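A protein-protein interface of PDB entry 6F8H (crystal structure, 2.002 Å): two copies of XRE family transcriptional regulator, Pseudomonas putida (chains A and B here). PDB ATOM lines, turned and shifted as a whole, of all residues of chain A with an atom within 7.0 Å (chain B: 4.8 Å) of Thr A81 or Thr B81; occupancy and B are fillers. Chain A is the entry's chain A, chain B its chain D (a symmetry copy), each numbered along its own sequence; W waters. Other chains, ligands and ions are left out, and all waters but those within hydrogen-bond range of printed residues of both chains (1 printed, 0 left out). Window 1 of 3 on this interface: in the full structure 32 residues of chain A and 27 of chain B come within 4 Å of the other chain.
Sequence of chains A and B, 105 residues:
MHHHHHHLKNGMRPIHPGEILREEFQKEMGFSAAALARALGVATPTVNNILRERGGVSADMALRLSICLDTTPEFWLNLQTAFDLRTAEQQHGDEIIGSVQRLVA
The backbone carbonyl oxygen (O) of Glu A74 sits close to the side-chain amide nitrogen (ND2) of Asn A78 (3.4 Å).
The side-chain hydroxyl (OG1) of Thr A81 lies within hydrogen-bond range of the backbone carbonyl oxygen (O) of Leu A77, at 3.4 Å.
O of Asn A78 lies within hydrogen-bond range of OG1 of Thr A81.
The backbone carbonyl oxygen (O) of Leu B77 sits at hydrogen-bond distance from the side-chain hydroxyl (OG1) of Thr B81, 3.3 Å away.
The side-chain amide nitrogen of Gln B80 lies within hydrogen-bond range of the side-chain carboxylate of Asp B84 (3.1 Å).
CB of Ala A59 touches O of Asp B84, 3.6 Å away.
Leu B85 touches Ala A59.
Pro A73 touches Leu B85.
Glu A74 touches Leu B85 (OE2 to CD1, 3.5 Å).
Thr B81 touches Leu A77.
CG of Leu B85 touches CD1 of Leu A77 (3.6 Å).
Asn A78 touches Asn B78 (OD1 to OD1, 3.8 Å).
CG2 of Thr B81 touches OD1 of Asn A78, at 3.96 Å.
Thr A81 touches Thr B81 (CG2 to OG1, 3.5 Å).
CD1 of Leu B77 touches CB of Leu A85, at 3.96 Å.
Printed residues of chain B within 4 Å of Thr A81: Leu B77 (3.98 Å) and Thr B81 (3.5 Å).
Thr B81 touches just these residues of chain A: Leu A77, Asn A78 and Thr A81.
Of the printed residues of chain A, Asn B78 touches Asn A78 (3.8 Å).
Of the printed residues of chain B, Asn A78 touches Asn B78 and Thr B81.
Printed residues of chain B within 4 Å of Glu A74: Leu B85.
Printed residues of chain A within 4 Å of Leu B77: Thr A81 and Leu A85.
The nearest printed residue of chain B that does not touch Thr A81 is Asn B78 (4.5 Å).
The nearest printed residue of chain A that does not touch Asn B78 is Thr A81 (4.5 Å).
Of the 16 printed residues of chain A, 7 touch a printed residue of chain B.
Along chain A the printed residues that touch a printed residue of chain B span positions 59 to 85.
Of the 9 printed residues of chain B, 5 touch a printed residue of chain A.
Among the printed residues, no Asp or Glu carboxylate lies within 4 Å of a Lys or Arg side-chain nitrogen of the other chain.
Leu A77 touches Thr B81, and with the chains exchanged Thr A81 touches Leu B77.
Asn B78 touches its own counterpart, Asn A78.
Asn A78 touches Thr B81, but with the chains exchanged Thr A81 does not touch Asn B78 (4.5 Å).
Thr A81 touches its own counterpart, Thr B81.
9 positions are printed for both chains.
Of the 11 pairs that touch across the chains among the printed residues, 6 have their exchanged pair printed and touching as well.
Water W1 lies within hydrogen-bond range of the side-chain amide oxygen (OD1) of Asn A78, the side-chain amide oxygen (OD1) of Asn B78, the side-chain hydroxyl (OG1) of Thr B81 and the side-chain hydroxyl (OG1) of Thr A81.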
ATOM      1  N   PRO A  17      18.799  13.287  -8.517  1.00  0.00           N
ATOM      2  CA  PRO A  17      18.156  14.593  -8.322  1.00  0.00           C
ATOM      3  C   PRO A  17      16.734  14.463  -7.800  1.00  0.00           C
ATOM      4  O   PRO A  17      16.282  15.311  -7.035  1.00  0.00           O
ATOM      5  CB  PRO A  17      18.174  15.211  -9.732  1.00  0.00           C
ATOM      6  CG  PRO A  17      19.367  14.581 -10.388  1.00  0.00           C
ATOM      7  CD  PRO A  17      19.433  13.168  -9.847  1.00  0.00           C
ATOM      8  N   ALA A  59      18.230  19.690 -19.587  1.00  0.00           N
ATOM      9  CA  ALA A  59      18.546  21.114 -19.493  1.00  0.00           C
ATOM     10  C   ALA A  59      17.256  21.948 -19.430  1.00  0.00           C
ATOM     11  O   ALA A  59      17.147  22.884 -18.631  1.00  0.00           O
ATOM     12  CB  ALA A  59      19.421  21.547 -20.660  1.00  0.00           C
ATOM     13  N   PRO A  73      19.795  26.750 -12.327  1.00  0.00           N
ATOM     14  CA  PRO A  73      19.580  25.504 -13.054  1.00  0.00           C
ATOM     15  C   PRO A  73      20.824  24.601 -12.977  1.00  0.00           C
ATOM     16  O   PRO A  73      20.688  23.389 -13.126  1.00  0.00           O
ATOM     17  CB  PRO A  73      19.287  25.975 -14.482  1.00  0.00           C
ATOM     18  CG  PRO A  73      20.018  27.259 -14.603  1.00  0.00           C
ATOM     19  CD  PRO A  73      19.978  27.903 -13.235  1.00  0.00           C
ATOM     20  N   GLU A  74      21.996  25.173 -12.695  1.00  0.00           N
ATOM     21  CA  GLU A  74      23.195  24.360 -12.496  1.00  0.00           C
ATOM     22  C   GLU A  74      23.019  23.401 -11.307  1.00  0.00           C
ATOM     23  O   GLU A  74      23.492  22.268 -11.356  1.00  0.00           O
ATOM     24  CB  GLU A  74      24.433  25.242 -12.297  1.00  0.00           C
ATOM     25  CG  GLU A  74      24.988  25.856 -13.602  1.00  0.00           C
ATOM     26  CD  GLU A  74      24.214  27.085 -14.069  1.00  0.00           C
ATOM     27  OE1 GLU A  74      23.258  27.505 -13.375  1.00  0.00           O
ATOM     28  OE2 GLU A  74      24.580  27.637 -15.130  1.00  0.00           O
ATOM     29  N   TRP A  76      20.538  21.655 -10.383  1.00  0.00           N
ATOM     30  CA  TRP A  76      19.903  20.416 -10.828  1.00  0.00           C
ATOM     31  C   TRP A  76      20.770  19.586 -11.773  1.00  0.00           C
ATOM     32  O   TRP A  76      20.878  18.378 -11.582  1.00  0.00           O
ATOM     33  CB  TRP A  76      18.536  20.726 -11.464  1.00  0.00           C
ATOM     34  CG  TRP A  76      17.619  21.332 -10.428  1.00  0.00           C
ATOM     35  CD1 TRP A  76      17.261  22.650 -10.307  1.00  0.00           C
ATOM     36  CD2 TRP A  76      17.012  20.649  -9.322  1.00  0.00           C
ATOM     37  NE1 TRP A  76      16.443  22.818  -9.212  1.00  0.00           N
ATOM     38  CE2 TRP A  76      16.270  21.603  -8.592  1.00  0.00           C
ATOM     39  CE3 TRP A  76      17.006  19.318  -8.887  1.00  0.00           C
ATOM     40  CZ2 TRP A  76      15.539  21.270  -7.442  1.00  0.00           C
ATOM     41  CZ3 TRP A  76      16.273  18.984  -7.743  1.00  0.00           C
ATOM     42  CH2 TRP A  76      15.547  19.954  -7.039  1.00  0.00           C
ATOM     43  N   LEU A  77      21.377  20.212 -12.780  1.00  0.00           N
ATOM     44  CA  LEU A  77      22.197  19.478 -13.741  1.00  0.00           C
ATOM     45  C   LEU A  77      23.481  18.950 -13.100  1.00  0.00           C
ATOM     46  O   LEU A  77      23.965  17.884 -13.472  1.00  0.00           O
ATOM     47  CB  LEU A  77      22.552  20.352 -14.950  1.00  0.00           C
ATOM     48  CG  LEU A  77      21.423  20.669 -15.935  1.00  0.00           C
ATOM     49  CD1 LEU A  77      21.969  21.010 -17.317  1.00  0.00           C
ATOM     50  CD2 LEU A  77      20.468  19.505 -16.024  1.00  0.00           C
ATOM     51  N   ASN A  78      24.035  19.693 -12.145  1.00  0.00           N
ATOM     52  CA  ASN A  78      25.183  19.182 -11.401  1.00  0.00           C
ATOM     53  C   ASN A  78      24.801  17.983 -10.528  1.00  0.00           C
ATOM     54  O   ASN A  78      25.597  17.070 -10.352  1.00  0.00           O
ATOM     55  CB  ASN A  78      25.823  20.289 -10.555  1.00  0.00           C
ATOM     56  CG  ASN A  78      26.478  21.360 -11.413  1.00  0.00           C
ATOM     57  OD1 ASN A  78      26.670  21.174 -12.615  1.00  0.00           O
ATOM     58  ND2 ASN A  78      26.844  22.473 -10.798  1.00  0.00           N
ATOM     59  N   LEU A  79      23.575  17.967 -10.009  1.00  0.00           N
ATOM     60  CA  LEU A  79      23.107  16.793  -9.279  1.00  0.00           C
ATOM     61  C   LEU A  79      23.004  15.617 -10.240  1.00  0.00           C
ATOM     62  O   LEU A  79      23.407  14.494  -9.920  1.00  0.00           O
ATOM     63  CB  LEU A  79      21.763  17.065  -8.595  1.00  0.00           C
ATOM     64  CG  LEU A  79      21.776  17.860  -7.283  1.00  0.00           C
ATOM     65  CD1 LEU A  79      20.342  18.162  -6.849  1.00  0.00           C
ATOM     66  CD2 LEU A  79      22.533  17.104  -6.169  1.00  0.00           C
ATOM     67  N   GLN A  80      22.490  15.892 -11.441  1.00  0.00           N
ATOM     68  CA  GLN A  80      22.355  14.874 -12.478  1.00  0.00           C
ATOM     69  C   GLN A  80      23.707  14.306 -12.925  1.00  0.00           C
ATOM     70  O   GLN A  80      23.860  13.098 -13.033  1.00  0.00           O
ATOM     71  CB  GLN A  80      21.613  15.436 -13.701  1.00  0.00           C
ATOM     72  CG  GLN A  80      21.318  14.379 -14.768  1.00  0.00           C
ATOM     73  CD  GLN A  80      20.398  13.279 -14.259  1.00  0.00           C
ATOM     74  OE1 GLN A  80      19.306  13.550 -13.742  1.00  0.00           O
ATOM     75  NE2 GLN A  80      20.833  12.028 -14.405  1.00  0.00           N
ATOM     76  N   THR A  81      24.686  15.161 -13.212  1.00  0.00           N
ATOM     77  CA  THR A  81      25.969  14.620 -13.674  1.00  0.00           C
ATOM     78  C   THR A  81      26.733  13.915 -12.540  1.00  0.00           C
ATOM     79  O   THR A  81      27.433  12.943 -12.791  1.00  0.00           O
ATOM     80  CB  THR A  81      26.874  15.691 -14.290  1.00  0.00           C
ATOM     81  OG1 THR A  81      27.138  16.694 -13.320  1.00  0.00           O
ATOM     82  CG2 THR A  81      26.216  16.332 -15.540  1.00  0.00           C
ATOM     83  N   ALA A  82      26.602  14.394 -11.307  1.00  0.00           N
ATOM     84  CA  ALA A  82      27.245  13.715 -10.188  1.00  0.00           C
ATOM     85  C   ALA A  82      26.659  12.309 -10.035  1.00  0.00           C
ATOM     86  O   ALA A  82      27.391  11.328  -9.862  1.00  0.00           O
ATOM     87  CB  ALA A  82      27.079  14.505  -8.902  1.00  0.00           C
ATOM     88  N   PHE A  83      25.338  12.217 -10.121  1.00  0.00           N
ATOM     89  CA  PHE A  83      24.666  10.929 -10.050  1.00  0.00           C
ATOM     90  C   PHE A  83      25.112  10.023 -11.183  1.00  0.00           C
ATOM     91  O   PHE A  83      25.428   8.859 -10.956  1.00  0.00           O
ATOM     92  CB  PHE A  83      23.149  11.102 -10.084  1.00  0.00           C
ATOM     93  CG  PHE A  83      22.394   9.816 -10.285  1.00  0.00           C
ATOM     94  CD1 PHE A  83      22.080   8.995  -9.200  1.00  0.00           C
ATOM     95  CD2 PHE A  83      21.989   9.430 -11.548  1.00  0.00           C
ATOM     96  CE1 PHE A  83      21.380   7.818  -9.385  1.00  0.00           C
ATOM     97  CE2 PHE A  83      21.296   8.259 -11.740  1.00  0.00           C
ATOM     98  CZ  PHE A  83      20.988   7.449 -10.656  1.00  0.00           C
ATOM     99  N   ASP A  84      25.116  10.560 -12.405  1.00  0.00           N
ATOM    100  CA  ASP A  84      25.517   9.789 -13.575  1.00  0.00           C
ATOM    101  C   ASP A  84      26.975   9.312 -13.513  1.00  0.00           C
ATOM    102  O   ASP A  84      27.299   8.200 -13.933  1.00  0.00           O
ATOM    103  CB  ASP A  84      25.293  10.623 -14.844  1.00  0.00           C
ATOM    104  CG  ASP A  84      23.817  10.761 -15.185  1.00  0.00           C
ATOM    105  OD1 ASP A  84      23.041   9.824 -14.878  1.00  0.00           O
ATOM    106  OD2 ASP A  84      23.434  11.800 -15.749  1.00  0.00           O
ATOM    107  N   LEU A  85      27.845  10.169 -13.002  1.00  0.00           N
ATOM    108  CA  LEU A  85      29.256   9.829 -12.873  1.00  0.00           C
ATOM    109  C   LEU A  85      29.457   8.738 -11.820  1.00  0.00           C
ATOM    110  O   LEU A  85      30.091   7.714 -12.071  1.00  0.00           O
ATOM    111  CB  LEU A  85      30.058  11.074 -12.516  1.00  0.00           C
ATOM    112  CG  LEU A  85      31.565  10.893 -12.315  1.00  0.00           C
ATOM    113  CD1 LEU A  85      32.206  10.399 -13.595  1.00  0.00           C
ATOM    114  CD2 LEU A  85      32.231  12.200 -11.861  1.00  0.00           C
ATOM    115  N   ARG A  86      28.891   8.963 -10.647  1.00  0.00           N
ATOM    116  CA  ARG A  86      28.997   7.995  -9.564  1.00  0.00           C
ATOM    117  C   ARG A  86      28.471   6.632 -10.040  1.00  0.00           C
ATOM    118  O   ARG A  86      29.059   5.586  -9.749  1.00  0.00           O
ATOM    119  CB  ARG A  86      28.238   8.495  -8.330  1.00  0.00           C
ATOM    120  CG  ARG A  86      28.443   7.650  -7.074  1.00  0.00           C
ATOM    121  CD  ARG A  86      29.836   7.822  -6.486  1.00  0.00           C
ATOM    122  NE  ARG A  86      30.318   6.553  -5.952  1.00  0.00           N
ATOM    123  CZ  ARG A  86      31.374   5.900  -6.424  1.00  0.00           C
ATOM    124  NH1 ARG A  86      32.080   6.411  -7.420  1.00  0.00           N
ATOM    125  NH2 ARG A  86      31.734   4.746  -5.887  1.00  0.00           N
ATOM    126  N   THR A  87      27.391   6.654 -10.818  1.00  0.00           N
ATOM    127  CA  THR A  87      26.814   5.428 -11.350  1.00  0.00           C
ATOM    128  C   THR A  87      27.751   4.734 -12.343  1.00  0.00           C
ATOM    129  O   THR A  87      27.988   3.526 -12.234  1.00  0.00           O
ATOM    130  CB  THR A  87      25.452   5.701 -12.017  1.00  0.00           C
ATOM    131  OG1 THR A  87      24.539   6.197 -11.038  1.00  0.00           O
ATOM    132  CG2 THR A  87      24.878   4.419 -12.614  1.00  0.00           C
ATOM    133  N   LEU B  77      32.020  16.914 -17.900  1.00  0.00           N
ATOM    134  CA  LEU B  77      30.584  16.970 -17.635  1.00  0.00           C
ATOM    135  C   LEU B  77      30.101  18.398 -17.408  1.00  0.00           C
ATOM    136  O   LEU B  77      28.986  18.745 -17.788  1.00  0.00           O
ATOM    137  CB  LEU B  77      30.228  16.101 -16.423  1.00  0.00           C
ATOM    138  CG  LEU B  77      30.505  14.615 -16.632  1.00  0.00           C
ATOM    139  CD1 LEU B  77      30.376  13.858 -15.316  1.00  0.00           C
ATOM    140  CD2 LEU B  77      29.553  14.054 -17.687  1.00  0.00           C
ATOM    141  N   ASN B  78      30.937  19.223 -16.789  1.00  0.00           N
ATOM    142  CA  ASN B  78      30.534  20.586 -16.496  1.00  0.00           C
ATOM    143  C   ASN B  78      30.574  21.406 -17.769  1.00  0.00           C
ATOM    144  O   ASN B  78      29.735  22.282 -17.965  1.00  0.00           O
ATOM    145  CB  ASN B  78      31.410  21.221 -15.398  1.00  0.00           C
ATOM    146  CG  ASN B  78      31.138  20.622 -14.013  1.00  0.00           C
ATOM    147  OD1 ASN B  78      30.111  19.981 -13.803  1.00  0.00           O
ATOM    148  ND2 ASN B  78      32.068  20.820 -13.067  1.00  0.00           N
ATOM    149  N   LEU B  79      31.528  21.115 -18.652  1.00  0.00           N
ATOM    150  CA  LEU B  79      31.503  21.741 -19.976  1.00  0.00           C
ATOM    151  C   LEU B  79      30.210  21.366 -20.691  1.00  0.00           C
ATOM    152  O   LEU B  79      29.572  22.215 -21.299  1.00  0.00           O
ATOM    153  CB  LEU B  79      32.699  21.326 -20.822  1.00  0.00           C
ATOM    154  CG  LEU B  79      34.034  21.945 -20.430  1.00  0.00           C
ATOM    155  CD1 LEU B  79      35.161  21.266 -21.207  1.00  0.00           C
ATOM    156  CD2 LEU B  79      34.000  23.471 -20.672  1.00  0.00           C
ATOM    157  N   GLN B  80      29.826  20.091 -20.595  1.00  0.00           N
ATOM    158  CA  GLN B  80      28.604  19.602 -21.231  1.00  0.00           C
ATOM    159  C   GLN B  80      27.351  20.268 -20.662  1.00  0.00           C
ATOM    160  O   GLN B  80      26.476  20.699 -21.419  1.00  0.00           O
ATOM    161  CB  GLN B  80      28.479  18.078 -21.080  1.00  0.00           C
ATOM    162  CG  GLN B  80      27.293  17.474 -21.859  1.00  0.00           C
ATOM    163  CD  GLN B  80      27.451  17.638 -23.368  1.00  0.00           C
ATOM    164  OE1 GLN B  80      28.490  17.300 -23.935  1.00  0.00           O
ATOM    165  NE2 GLN B  80      26.426  18.178 -24.018  1.00  0.00           N
ATOM    166  N   THR B  81      27.271  20.325 -19.335  1.00  0.00           N
ATOM    167  CA  THR B  81      26.174  20.981 -18.616  1.00  0.00           C
ATOM    168  C   THR B  81      26.018  22.461 -19.049  1.00  0.00           C
ATOM    169  O   THR B  81      24.916  22.928 -19.379  1.00  0.00           O
ATOM    170  CB  THR B  81      26.402  20.902 -17.091  1.00  0.00           C
ATOM    171  OG1 THR B  81      26.018  19.606 -16.621  1.00  0.00           O
ATOM    172  CG2 THR B  81      25.582  21.950 -16.342  1.00  0.00           C
ATOM    173  N   ALA B  82      27.126  23.182 -19.045  1.00  0.00           N
ATOM    174  CA  ALA B  82      27.149  24.581 -19.473  1.00  0.00           C
ATOM    175  C   ALA B  82      26.656  24.737 -20.912  1.00  0.00           C
ATOM    176  O   ALA B  82      25.851  25.627 -21.209  1.00  0.00           O
ATOM    177  CB  ALA B  82      28.546  25.142 -19.331  1.00  0.00           C
ATOM    178  N   PHE B  83      27.129  23.862 -21.794  1.00  0.00           N
ATOM    179  CA  PHE B  83      26.728  23.914 -23.203  1.00  0.00           C
ATOM    180  C   PHE B  83      25.235  23.665 -23.379  1.00  0.00           C
ATOM    181  O   PHE B  83      24.575  24.351 -24.157  1.00  0.00           O
ATOM    182  CB  PHE B  83      27.521  22.905 -24.037  1.00  0.00           C
ATOM    183  CG  PHE B  83      27.015  22.747 -25.441  1.00  0.00           C
ATOM    184  CD1 PHE B  83      27.380  23.652 -26.428  1.00  0.00           C
ATOM    185  CD2 PHE B  83      26.169  21.698 -25.776  1.00  0.00           C
ATOM    186  CE1 PHE B  83      26.911  23.526 -27.709  1.00  0.00           C
ATOM    187  CE2 PHE B  83      25.695  21.562 -27.075  1.00  0.00           C
ATOM    188  CZ  PHE B  83      26.077  22.481 -28.044  1.00  0.00           C
ATOM    189  N   ASP B  84      24.709  22.678 -22.655  1.00  0.00           N
ATOM    190  CA  ASP B  84      23.307  22.319 -22.777  1.00  0.00           C
ATOM    191  C   ASP B  84      22.407  23.389 -22.185  1.00  0.00           C
ATOM    192  O   ASP B  84      21.356  23.677 -22.741  1.00  0.00           O
ATOM    193  CB  ASP B  84      23.038  20.956 -22.120  1.00  0.00           C
ATOM    194  CG  ASP B  84      23.540  19.812 -22.968  1.00  0.00           C
ATOM    195  OD1 ASP B  84      23.652  20.017 -24.193  1.00  0.00           O
ATOM    196  OD2 ASP B  84      23.825  18.716 -22.435  1.00  0.00           O
ATOM    197  N   LEU B  85      22.817  23.983 -21.067  1.00  0.00           N
ATOM    198  CA  LEU B  85      22.028  25.054 -20.462  1.00  0.00           C
ATOM    199  C   LEU B  85      22.004  26.309 -21.325  1.00  0.00           C
ATOM    200  O   LEU B  85      20.954  26.893 -21.547  1.00  0.00           O
ATOM    201  CB  LEU B  85      22.559  25.422 -19.083  1.00  0.00           C
ATOM    202  CG  LEU B  85      22.134  24.514 -17.939  1.00  0.00           C
ATOM    203  CD1 LEU B  85      22.720  25.032 -16.632  1.00  0.00           C
ATOM    204  CD2 LEU B  85      20.609  24.412 -17.873  1.00  0.00           C
HETATM  205  O   HOH W   1      27.541  19.338 -14.369  1.00  0.00           O
